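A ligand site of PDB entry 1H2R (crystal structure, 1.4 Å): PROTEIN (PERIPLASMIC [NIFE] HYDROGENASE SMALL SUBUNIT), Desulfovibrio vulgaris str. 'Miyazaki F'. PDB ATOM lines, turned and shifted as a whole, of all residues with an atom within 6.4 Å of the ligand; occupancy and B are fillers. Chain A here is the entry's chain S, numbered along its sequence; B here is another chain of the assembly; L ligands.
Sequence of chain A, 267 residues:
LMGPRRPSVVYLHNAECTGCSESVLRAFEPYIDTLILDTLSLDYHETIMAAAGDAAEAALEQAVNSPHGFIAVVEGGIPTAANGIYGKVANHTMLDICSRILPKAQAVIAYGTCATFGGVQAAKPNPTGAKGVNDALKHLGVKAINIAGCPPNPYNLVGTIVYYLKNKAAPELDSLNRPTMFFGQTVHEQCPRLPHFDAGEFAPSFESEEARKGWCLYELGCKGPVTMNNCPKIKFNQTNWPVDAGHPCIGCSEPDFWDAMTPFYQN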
ATOM      1  N   ALA A  15      32.453   0.635   5.419  1.00  0.00           N
ATOM      2  CA  ALA A  15      33.379   1.432   4.621  1.00  0.00           C
ATOM      3  C   ALA A  15      32.540   1.930   3.433  1.00  0.00           C
ATOM      4  O   ALA A  15      32.337   1.194   2.462  1.00  0.00           O
ATOM      5  CB  ALA A  15      34.569   0.590   4.149  1.00  0.00           C
ATOM      6  N   GLU A  16      32.081   3.181   3.528  1.00  0.00           N
ATOM      7  CA  GLU A  16      31.193   3.786   2.535  1.00  0.00           C
ATOM      8  C   GLU A  16      31.411   5.284   2.352  1.00  0.00           C
ATOM      9  O   GLU A  16      32.098   5.912   3.162  1.00  0.00           O
ATOM     10  CB  GLU A  16      29.738   3.549   2.974  1.00  0.00           C
ATOM     11  CG  GLU A  16      29.464   3.735   4.493  1.00  0.00           C
ATOM     12  CD  GLU A  16      29.201   5.180   4.916  1.00  0.00           C
ATOM     13  OE1 GLU A  16      28.513   5.891   4.154  1.00  0.00           O
ATOM     14  OE2 GLU A  16      29.657   5.597   6.000  1.00  0.00           O
ATOM     15  N   CYS A  17      30.769   5.850   1.334  1.00  0.00           N
ATOM     16  CA  CYS A  17      30.881   7.274   1.020  1.00  0.00           C
ATOM     17  C   CYS A  17      29.599   8.055   1.338  1.00  0.00           C
ATOM     18  O   CYS A  17      29.552   9.288   1.172  1.00  0.00           O
ATOM     19  CB  CYS A  17      31.223   7.457  -0.479  1.00  0.00           C
ATOM     20  SG  CYS A  17      29.836   7.274  -1.672  1.00  0.00           S
ATOM     21  N   THR A  18      28.540   7.331   1.719  1.00  0.00           N
ATOM     22  CA  THR A  18      27.224   7.894   2.042  1.00  0.00           C
ATOM     23  C   THR A  18      26.342   8.189   0.821  1.00  0.00           C
ATOM     24  O   THR A  18      25.179   8.620   0.947  1.00  0.00           O
ATOM     25  CB  THR A  18      27.359   9.102   3.019  1.00  0.00           C
ATOM     26  OG1 THR A  18      28.191   8.720   4.123  1.00  0.00           O
ATOM     27  CG2 THR A  18      25.993   9.492   3.605  1.00  0.00           C
ATOM     28  N   GLY A  19      26.867   7.899  -0.368  1.00  0.00           N
ATOM     29  CA  GLY A  19      26.113   8.094  -1.603  1.00  0.00           C
ATOM     30  C   GLY A  19      24.894   7.178  -1.629  1.00  0.00           C
ATOM     31  O   GLY A  19      23.847   7.545  -2.177  1.00  0.00           O
ATOM     32  N   CYS A  20      25.014   5.995  -1.044  1.00  0.00           N
ATOM     33  CA  CYS A  20      23.887   5.077  -1.002  1.00  0.00           C
ATOM     34  C   CYS A  20      22.790   5.653  -0.062  1.00  0.00           C
ATOM     35  O   CYS A  20      21.594   5.617  -0.388  1.00  0.00           O
ATOM     36  CB  CYS A  20      24.357   3.662  -0.624  1.00  0.00           C
ATOM     37  SG  CYS A  20      25.238   2.751  -1.967  1.00  0.00           S
ATOM     38  N   SER A  21      23.189   6.243   1.068  1.00  0.00           N
ATOM     39  CA  SER A  21      22.191   6.844   1.967  1.00  0.00           C
ATOM     40  C   SER A  21      21.470   7.966   1.238  1.00  0.00           C
ATOM     41  O   SER A  21      20.250   8.046   1.256  1.00  0.00           O
ATOM     42  CB  SER A  21      22.849   7.406   3.227  1.00  0.00           C
ATOM     43  OG  SER A  21      23.043   6.385   4.190  1.00  0.00           O
ATOM     44  N   GLU A  75      25.207  -0.614   4.216  1.00  0.00           N
ATOM     45  CA  GLU A  75      25.902   0.205   3.225  1.00  0.00           C
ATOM     46  C   GLU A  75      27.396   0.127   3.518  1.00  0.00           C
ATOM     47  O   GLU A  75      27.804   0.232   4.688  1.00  0.00           O
ATOM     48  CB  GLU A  75      25.403   1.657   3.313  1.00  0.00           C
ATOM     49  CG  GLU A  75      26.186   2.664   2.489  1.00  0.00           C
ATOM     50  CD  GLU A  75      25.579   4.074   2.514  1.00  0.00           C
ATOM     51  OE1 GLU A  75      24.591   4.288   3.250  1.00  0.00           O
ATOM     52  OE2 GLU A  75      26.097   4.949   1.793  1.00  0.00           O
ATOM     53  N   GLY A  76      28.208  -0.104   2.484  1.00  0.00           N
ATOM     54  CA  GLY A  76      29.659  -0.182   2.622  1.00  0.00           C
ATOM     55  C   GLY A  76      30.287  -1.553   2.798  1.00  0.00           C
ATOM     56  O   GLY A  76      29.651  -2.498   3.268  1.00  0.00           O
ATOM     57  N   GLY A  77      31.561  -1.651   2.417  1.00  0.00           N
ATOM     58  CA  GLY A  77      32.301  -2.901   2.533  1.00  0.00           C
ATOM     59  C   GLY A  77      32.902  -3.111   3.911  1.00  0.00           C
ATOM     60  O   GLY A  77      33.039  -2.159   4.675  1.00  0.00           O
ATOM     61  N   TYR A 111      23.023  -3.047   0.357  1.00  0.00           N
ATOM     62  CA  TYR A 111      22.664  -1.974  -0.564  1.00  0.00           C
ATOM     63  C   TYR A 111      23.920  -1.230  -1.032  1.00  0.00           C
ATOM     64  O   TYR A 111      24.629  -0.623  -0.220  1.00  0.00           O
ATOM     65  CB  TYR A 111      21.646  -1.039   0.141  1.00  0.00           C
ATOM     66  CG  TYR A 111      21.017   0.051  -0.716  1.00  0.00           C
ATOM     67  CD1 TYR A 111      20.188  -0.270  -1.784  1.00  0.00           C
ATOM     68  CD2 TYR A 111      21.310   1.400  -0.508  1.00  0.00           C
ATOM     69  CE1 TYR A 111      19.678   0.712  -2.639  1.00  0.00           C
ATOM     70  CE2 TYR A 111      20.786   2.397  -1.350  1.00  0.00           C
ATOM     71  CZ  TYR A 111      19.971   2.032  -2.421  1.00  0.00           C
ATOM     72  OH  TYR A 111      19.461   2.972  -3.286  1.00  0.00           O
ATOM     73  N   GLY A 112      24.203  -1.332  -2.333  1.00  0.00           N
ATOM     74  CA  GLY A 112      25.356  -0.674  -2.938  1.00  0.00           C
ATOM     75  C   GLY A 112      26.459  -1.678  -3.253  1.00  0.00           C
ATOM     76  O   GLY A 112      26.692  -2.604  -2.473  1.00  0.00           O
ATOM     77  N   THR A 113      27.170  -1.447  -4.357  1.00  0.00           N
ATOM     78  CA  THR A 113      28.269  -2.320  -4.772  1.00  0.00           C
ATOM     79  C   THR A 113      29.358  -2.560  -3.693  1.00  0.00           C
ATOM     80  O   THR A 113      29.991  -3.625  -3.658  1.00  0.00           O
ATOM     81  CB  THR A 113      28.873  -1.831  -6.101  1.00  0.00           C
ATOM     82  OG1 THR A 113      27.885  -1.998  -7.131  1.00  0.00           O
ATOM     83  CG2 THR A 113      30.160  -2.627  -6.489  1.00  0.00           C
ATOM     84  N   CYS A 114      29.543  -1.607  -2.795  1.00  0.00           N
ATOM     85  CA  CYS A 114      30.510  -1.785  -1.719  1.00  0.00           C
ATOM     86  C   CYS A 114      30.070  -2.877  -0.769  1.00  0.00           C
ATOM     87  O   CYS A 114      30.876  -3.742  -0.392  1.00  0.00           O
ATOM     88  CB  CYS A 114      30.700  -0.507  -0.915  1.00  0.00           C
ATOM     89  SG  CYS A 114      31.598   0.767  -1.808  1.00  0.00           S
ATOM     90  N   ALA A 115      28.795  -2.835  -0.353  1.00  0.00           N
ATOM     91  CA  ALA A 115      28.210  -3.806   0.559  1.00  0.00           C
ATOM     92  C   ALA A 115      28.010  -5.154  -0.108  1.00  0.00           C
ATOM     93  O   ALA A 115      28.169  -6.210   0.519  1.00  0.00           O
ATOM     94  CB  ALA A 115      26.886  -3.290   1.122  1.00  0.00           C
ATOM     95  N   GLY A 119      33.466  -3.292  -3.414  1.00  0.00           N
ATOM     96  CA  GLY A 119      33.478  -1.910  -3.876  1.00  0.00           C
ATOM     97  C   GLY A 119      34.794  -1.199  -4.094  1.00  0.00           C
ATOM     98  O   GLY A 119      35.854  -1.820  -4.230  1.00  0.00           O
ATOM     99  N   VAL A 120      34.724   0.127  -4.056  1.00  0.00           N
ATOM    100  CA  VAL A 120      35.881   0.973  -4.311  1.00  0.00           C
ATOM    101  C   VAL A 120      37.109   0.671  -3.450  1.00  0.00           C
ATOM    102  O   VAL A 120      38.206   0.567  -3.995  1.00  0.00           O
ATOM    103  CB  VAL A 120      35.500   2.490  -4.349  1.00  0.00           C
ATOM    104  CG1 VAL A 120      35.283   3.064  -2.947  1.00  0.00           C
ATOM    105  CG2 VAL A 120      36.555   3.292  -5.115  1.00  0.00           C
ATOM    106  N   GLN A 121      36.932   0.496  -2.143  1.00  0.00           N
ATOM    107  CA  GLN A 121      38.088   0.206  -1.294  1.00  0.00           C
ATOM    108  C   GLN A 121      38.676  -1.221  -1.495  1.00  0.00           C
ATOM    109  O   GLN A 121      39.796  -1.495  -1.046  1.00  0.00           O
ATOM    110  CB  GLN A 121      37.769   0.471   0.189  1.00  0.00           C
ATOM    111  CG  GLN A 121      36.571  -0.304   0.779  1.00  0.00           C
ATOM    112  CD  GLN A 121      35.259   0.418   0.557  1.00  0.00           C
ATOM    113  OE1 GLN A 121      35.195   1.628   0.679  1.00  0.00           O
ATOM    114  NE2 GLN A 121      34.220  -0.316   0.184  1.00  0.00           N
ATOM    115  N   GLY A 149      25.009  -1.398  -7.501  1.00  0.00           N
ATOM    116  CA  GLY A 149      24.987  -0.076  -8.119  1.00  0.00           C
ATOM    117  C   GLY A 149      25.831   0.882  -7.280  1.00  0.00           C
ATOM    118  O   GLY A 149      25.939   0.688  -6.080  1.00  0.00           O
ATOM    119  N   CYS A 150      26.357   1.946  -7.895  1.00  0.00           N
ATOM    120  CA  CYS A 150      27.216   2.882  -7.175  1.00  0.00           C
ATOM    121  C   CYS A 150      26.812   4.353  -7.328  1.00  0.00           C
ATOM    122  O   CYS A 150      27.519   5.143  -7.953  1.00  0.00           O
ATOM    123  CB  CYS A 150      28.664   2.666  -7.655  1.00  0.00           C
ATOM    124  SG  CYS A 150      29.996   3.242  -6.555  1.00  0.00           S
ATOM    125  N   PRO A 151      25.703   4.765  -6.689  1.00  0.00           N
ATOM    126  CA  PRO A 151      24.799   3.993  -5.852  1.00  0.00           C
ATOM    127  C   PRO A 151      23.687   3.348  -6.674  1.00  0.00           C
ATOM    128  O   PRO A 151      23.542   3.620  -7.868  1.00  0.00           O
ATOM    129  CB  PRO A 151      24.234   5.061  -4.914  1.00  0.00           C
ATOM    130  CG  PRO A 151      24.063   6.237  -5.831  1.00  0.00           C
ATOM    131  CD  PRO A 151      25.338   6.204  -6.668  1.00  0.00           C
ATOM    132  N   PRO A 152      22.917   2.435  -6.076  1.00  0.00           N
ATOM    133  CA  PRO A 152      21.830   1.792  -6.842  1.00  0.00           C
ATOM    134  C   PRO A 152      20.647   2.758  -7.061  1.00  0.00           C
ATOM    135  O   PRO A 152      20.608   3.858  -6.493  1.00  0.00           O
ATOM    136  CB  PRO A 152      21.393   0.645  -5.908  1.00  0.00           C
ATOM    137  CG  PRO A 152      22.608   0.433  -5.006  1.00  0.00           C
ATOM    138  CD  PRO A 152      23.112   1.797  -4.764  1.00  0.00           C
ATOM    139  N   TRP A 258      35.791  -2.017 -10.607  1.00  0.00           N
ATOM    140  CA  TRP A 258      36.932  -1.091 -10.557  1.00  0.00           C
ATOM    141  C   TRP A 258      38.181  -1.650 -11.241  1.00  0.00           C
ATOM    142  O   TRP A 258      38.967  -0.890 -11.809  1.00  0.00           O
ATOM    143  CB  TRP A 258      37.231  -0.705  -9.109  1.00  0.00           C
ATOM    144  CG  TRP A 258      36.071   0.011  -8.467  1.00  0.00           C
ATOM    145  CD1 TRP A 258      35.202  -0.492  -7.541  1.00  0.00           C
ATOM    146  CD2 TRP A 258      35.664   1.373  -8.706  1.00  0.00           C
ATOM    147  NE1 TRP A 258      34.284   0.474  -7.184  1.00  0.00           N
ATOM    148  CE2 TRP A 258      34.538   1.627  -7.878  1.00  0.00           C
ATOM    149  CE3 TRP A 258      36.138   2.396  -9.543  1.00  0.00           C
ATOM    150  CZ2 TRP A 258      33.890   2.867  -7.854  1.00  0.00           C
ATOM    151  CZ3 TRP A 258      35.478   3.638  -9.511  1.00  0.00           C
ATOM    152  CH2 TRP A 258      34.367   3.850  -8.672  1.00  0.00           C
ATOM    153  N   ARG B  41      40.189   4.111   3.926  1.00  0.00           N
ATOM    154  CA  ARG B  41      39.910   3.336   2.705  1.00  0.00           C
ATOM    155  C   ARG B  41      41.160   3.259   1.817  1.00  0.00           C
ATOM    156  O   ARG B  41      41.444   2.219   1.213  1.00  0.00           O
ATOM    157  CB  ARG B  41      38.688   3.909   1.956  1.00  0.00           C
ATOM    158  CG  ARG B  41      37.342   3.589   2.649  1.00  0.00           C
ATOM    159  CD  ARG B  41      36.138   4.255   1.960  1.00  0.00           C
ATOM    160  NE  ARG B  41      36.264   5.707   2.005  1.00  0.00           N
ATOM    161  CZ  ARG B  41      35.666   6.561   1.181  1.00  0.00           C
ATOM    162  NH1 ARG B  41      34.863   6.118   0.219  1.00  0.00           N
ATOM    163  NH2 ARG B  41      35.925   7.867   1.282  1.00  0.00           N
ATOM    164  N   ARG B  61      33.832   8.770  -5.592  1.00  0.00           N
ATOM    165  CA  ARG B  61      33.427   7.820  -4.546  1.00  0.00           C
ATOM    166  C   ARG B  61      34.048   8.141  -3.179  1.00  0.00           C
ATOM    167  O   ARG B  61      33.879   7.393  -2.227  1.00  0.00           O
ATOM    168  CB  ARG B  61      33.782   6.382  -4.972  1.00  0.00           C
ATOM    169  CG  ARG B  61      32.621   5.500  -5.474  1.00  0.00           C
ATOM    170  CD  ARG B  61      31.585   6.131  -6.415  1.00  0.00           C
ATOM    171  NE  ARG B  61      32.069   6.617  -7.689  1.00  0.00           N
ATOM    172  CZ  ARG B  61      31.384   6.561  -8.849  1.00  0.00           C
ATOM    173  NH1 ARG B  61      30.169   6.029  -8.911  1.00  0.00           N
ATOM    174  NH2 ARG B  61      31.852   7.205  -9.905  1.00  0.00           N
ATOM    175  N   THR B  62      34.831   9.219  -3.113  1.00  0.00           N
ATOM    176  CA  THR B  62      35.389   9.680  -1.853  1.00  0.00           C
ATOM    177  C   THR B  62      34.177  10.077  -0.988  1.00  0.00           C
ATOM    178  O   THR B  62      34.150   9.819   0.224  1.00  0.00           O
ATOM    179  CB  THR B  62      36.256  10.962  -2.076  1.00  0.00           C
ATOM    180  OG1 THR B  62      37.467  10.619  -2.783  1.00  0.00           O
ATOM    181  CG2 THR B  62      36.642  11.624  -0.761  1.00  0.00           C
ATOM    182  N   CYS B  63      33.146  10.667  -1.625  1.00  0.00           N
ATOM    183  CA  CYS B  63      31.961  11.108  -0.901  1.00  0.00           C
ATOM    184  C   CYS B  63      30.668  11.247  -1.735  1.00  0.00           C
ATOM    185  O   CYS B  63      30.674  11.807  -2.824  1.00  0.00           O
ATOM    186  CB  CYS B  63      32.244  12.455  -0.223  1.00  0.00           C
ATOM    187  SG  CYS B  63      30.857  13.101   0.798  1.00  0.00           S
ATOM    188  N   GLY B  64      29.566  10.767  -1.145  1.00  0.00           N
ATOM    189  CA  GLY B  64      28.254  10.847  -1.765  1.00  0.00           C
ATOM    190  C   GLY B  64      27.420  12.059  -1.340  1.00  0.00           C
ATOM    191  O   GLY B  64      26.412  12.343  -1.986  1.00  0.00           O
ATOM    192  N   PRO B 216      22.659  10.687  -6.621  1.00  0.00           N
ATOM    193  CA  PRO B 216      24.103  10.903  -6.459  1.00  0.00           C
ATOM    194  C   PRO B 216      24.997  10.337  -7.557  1.00  0.00           C
ATOM    195  O   PRO B 216      24.633   9.416  -8.288  1.00  0.00           O
ATOM    196  CB  PRO B 216      24.403  10.202  -5.130  1.00  0.00           C
ATOM    197  CG  PRO B 216      23.059  10.085  -4.416  1.00  0.00           C
ATOM    198  CD  PRO B 216      22.151   9.788  -5.584  1.00  0.00           C
ATOM    199  N   HIS B 217      26.214  10.892  -7.597  1.00  0.00           N
ATOM    200  CA  HIS B 217      27.287  10.508  -8.501  1.00  0.00           C
ATOM    201  C   HIS B 217      27.044  10.758  -9.973  1.00  0.00           C
ATOM    202  O   HIS B 217      26.670   9.880 -10.752  1.00  0.00           O
ATOM    203  CB  HIS B 217      27.773   9.091  -8.165  1.00  0.00           C
ATOM    204  CG  HIS B 217      28.488   9.020  -6.836  1.00  0.00           C
ATOM    205  ND1 HIS B 217      28.718   7.841  -6.155  1.00  0.00           N
ATOM    206  CD2 HIS B 217      28.996  10.005  -6.060  1.00  0.00           C
ATOM    207  CE1 HIS B 217      29.355   8.102  -5.031  1.00  0.00           C
ATOM    208  NE2 HIS B 217      29.531   9.409  -4.942  1.00  0.00           N
HETATM  209 FE1  LIG L   1      29.495   5.045  -2.163  1.00  0.00          FE
HETATM  210 FE2  LIG L   1      30.008   2.412  -2.104  1.00  0.00          FE
HETATM  211 FE3  LIG L   1      29.288   3.568  -4.375  1.00  0.00          FE
HETATM  212 FE4  LIG L   1      27.407   3.353  -2.379  1.00  0.00          FE
HETATM  213  S1  LIG L   1      28.370   1.586  -3.565  1.00  0.00           S
HETATM  214  S2  LIG L   1      27.773   5.205  -3.739  1.00  0.00           S
HETATM  215  S3  LIG L   1      28.811   3.579  -0.494  1.00  0.00           S
HETATM  216  S4  LIG L   1      31.230   3.996  -3.200  1.00  0.00           S
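An iron atom (FE4) of the ligand is bound by the side-chain sulfur of Cys 20 (2.3 Å).
N of Cys 114 sits close to S1 of the ligand, at 3.5 Å.
An iron atom (FE2) of the ligand is bound by the side-chain sulfur (SG) of Cys 114 (2.3 Å).
S3 of the ligand sits close to N of Cys 17 (3.5 Å).
FE1 of the ligand is bound by SG of Cys 17, 2.3 Å away.
SG of Cys 150 binds FE3 of the ligand, 2.3 Å away.
A sulfur (S1) of the ligand sits close to the backbone NH (N) of Thr 113, at 3.4 Å.
A sulfur (S2) of the ligand sits close to a ring nitrogen (ND1) of His 217 of chain B (3.7 Å).
SG of Cys 114 sits close to NE2 of Gln 121 (3.5 Å).
N of Gly 19 lies close to SG of Cys 17, 3.3 Å away.
NH1 of Arg 61 of chain B lies within hydrogen-bond range of O of Cys 150, 3.0 Å away.
The backbone carbonyl oxygen (O) of Cys 150 is in hydrogen-bond range of a ring nitrogen (ND1) of His 217 of chain B, at 3.5 Å.
O of Arg 61 of chain B is in hydrogen-bond range of NH1 of Arg 41 of chain B, 2.9 Å away.
The side-chain hydroxyl of Thr 113 is in hydrogen-bond range of the backbone NH of Gly 149, at 3.0 Å.
The backbone carbonyl oxygen (O) of Thr 113 sits at hydrogen-bond distance from the backbone NH (N) of Gly 119, at 3.5 Å.
A ring nitrogen (NE2) of His 217 of chain B is in hydrogen-bond range of the backbone carbonyl oxygen of Cys 63 of chain B, 3.4 Å away.
A sulfur (S1) of the ligand sits close to the backbone carbonyl oxygen (O) of Gly 149 (3.6 Å).
The backbone nitrogen of Pro 151 sits close to a sulfur (S2) of the ligand (3.6 Å).
Merely in contact with the ligand: Arg 61 of chain B, Glu 16, Gly 112, Glu 75 and Gly 19.
Hydrophobic or aromatic side chains that line the ligand: Pro 151 and His 217 of chain B.
Within 4 Å of the ligand: Glu 16, Cys 17, Gly 19, Cys 20, Glu 75, Gly 112, Thr 113, Cys 114, Gly 149, Cys 150, Pro 151, Arg 61 of chain B and His 217 of chain B.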
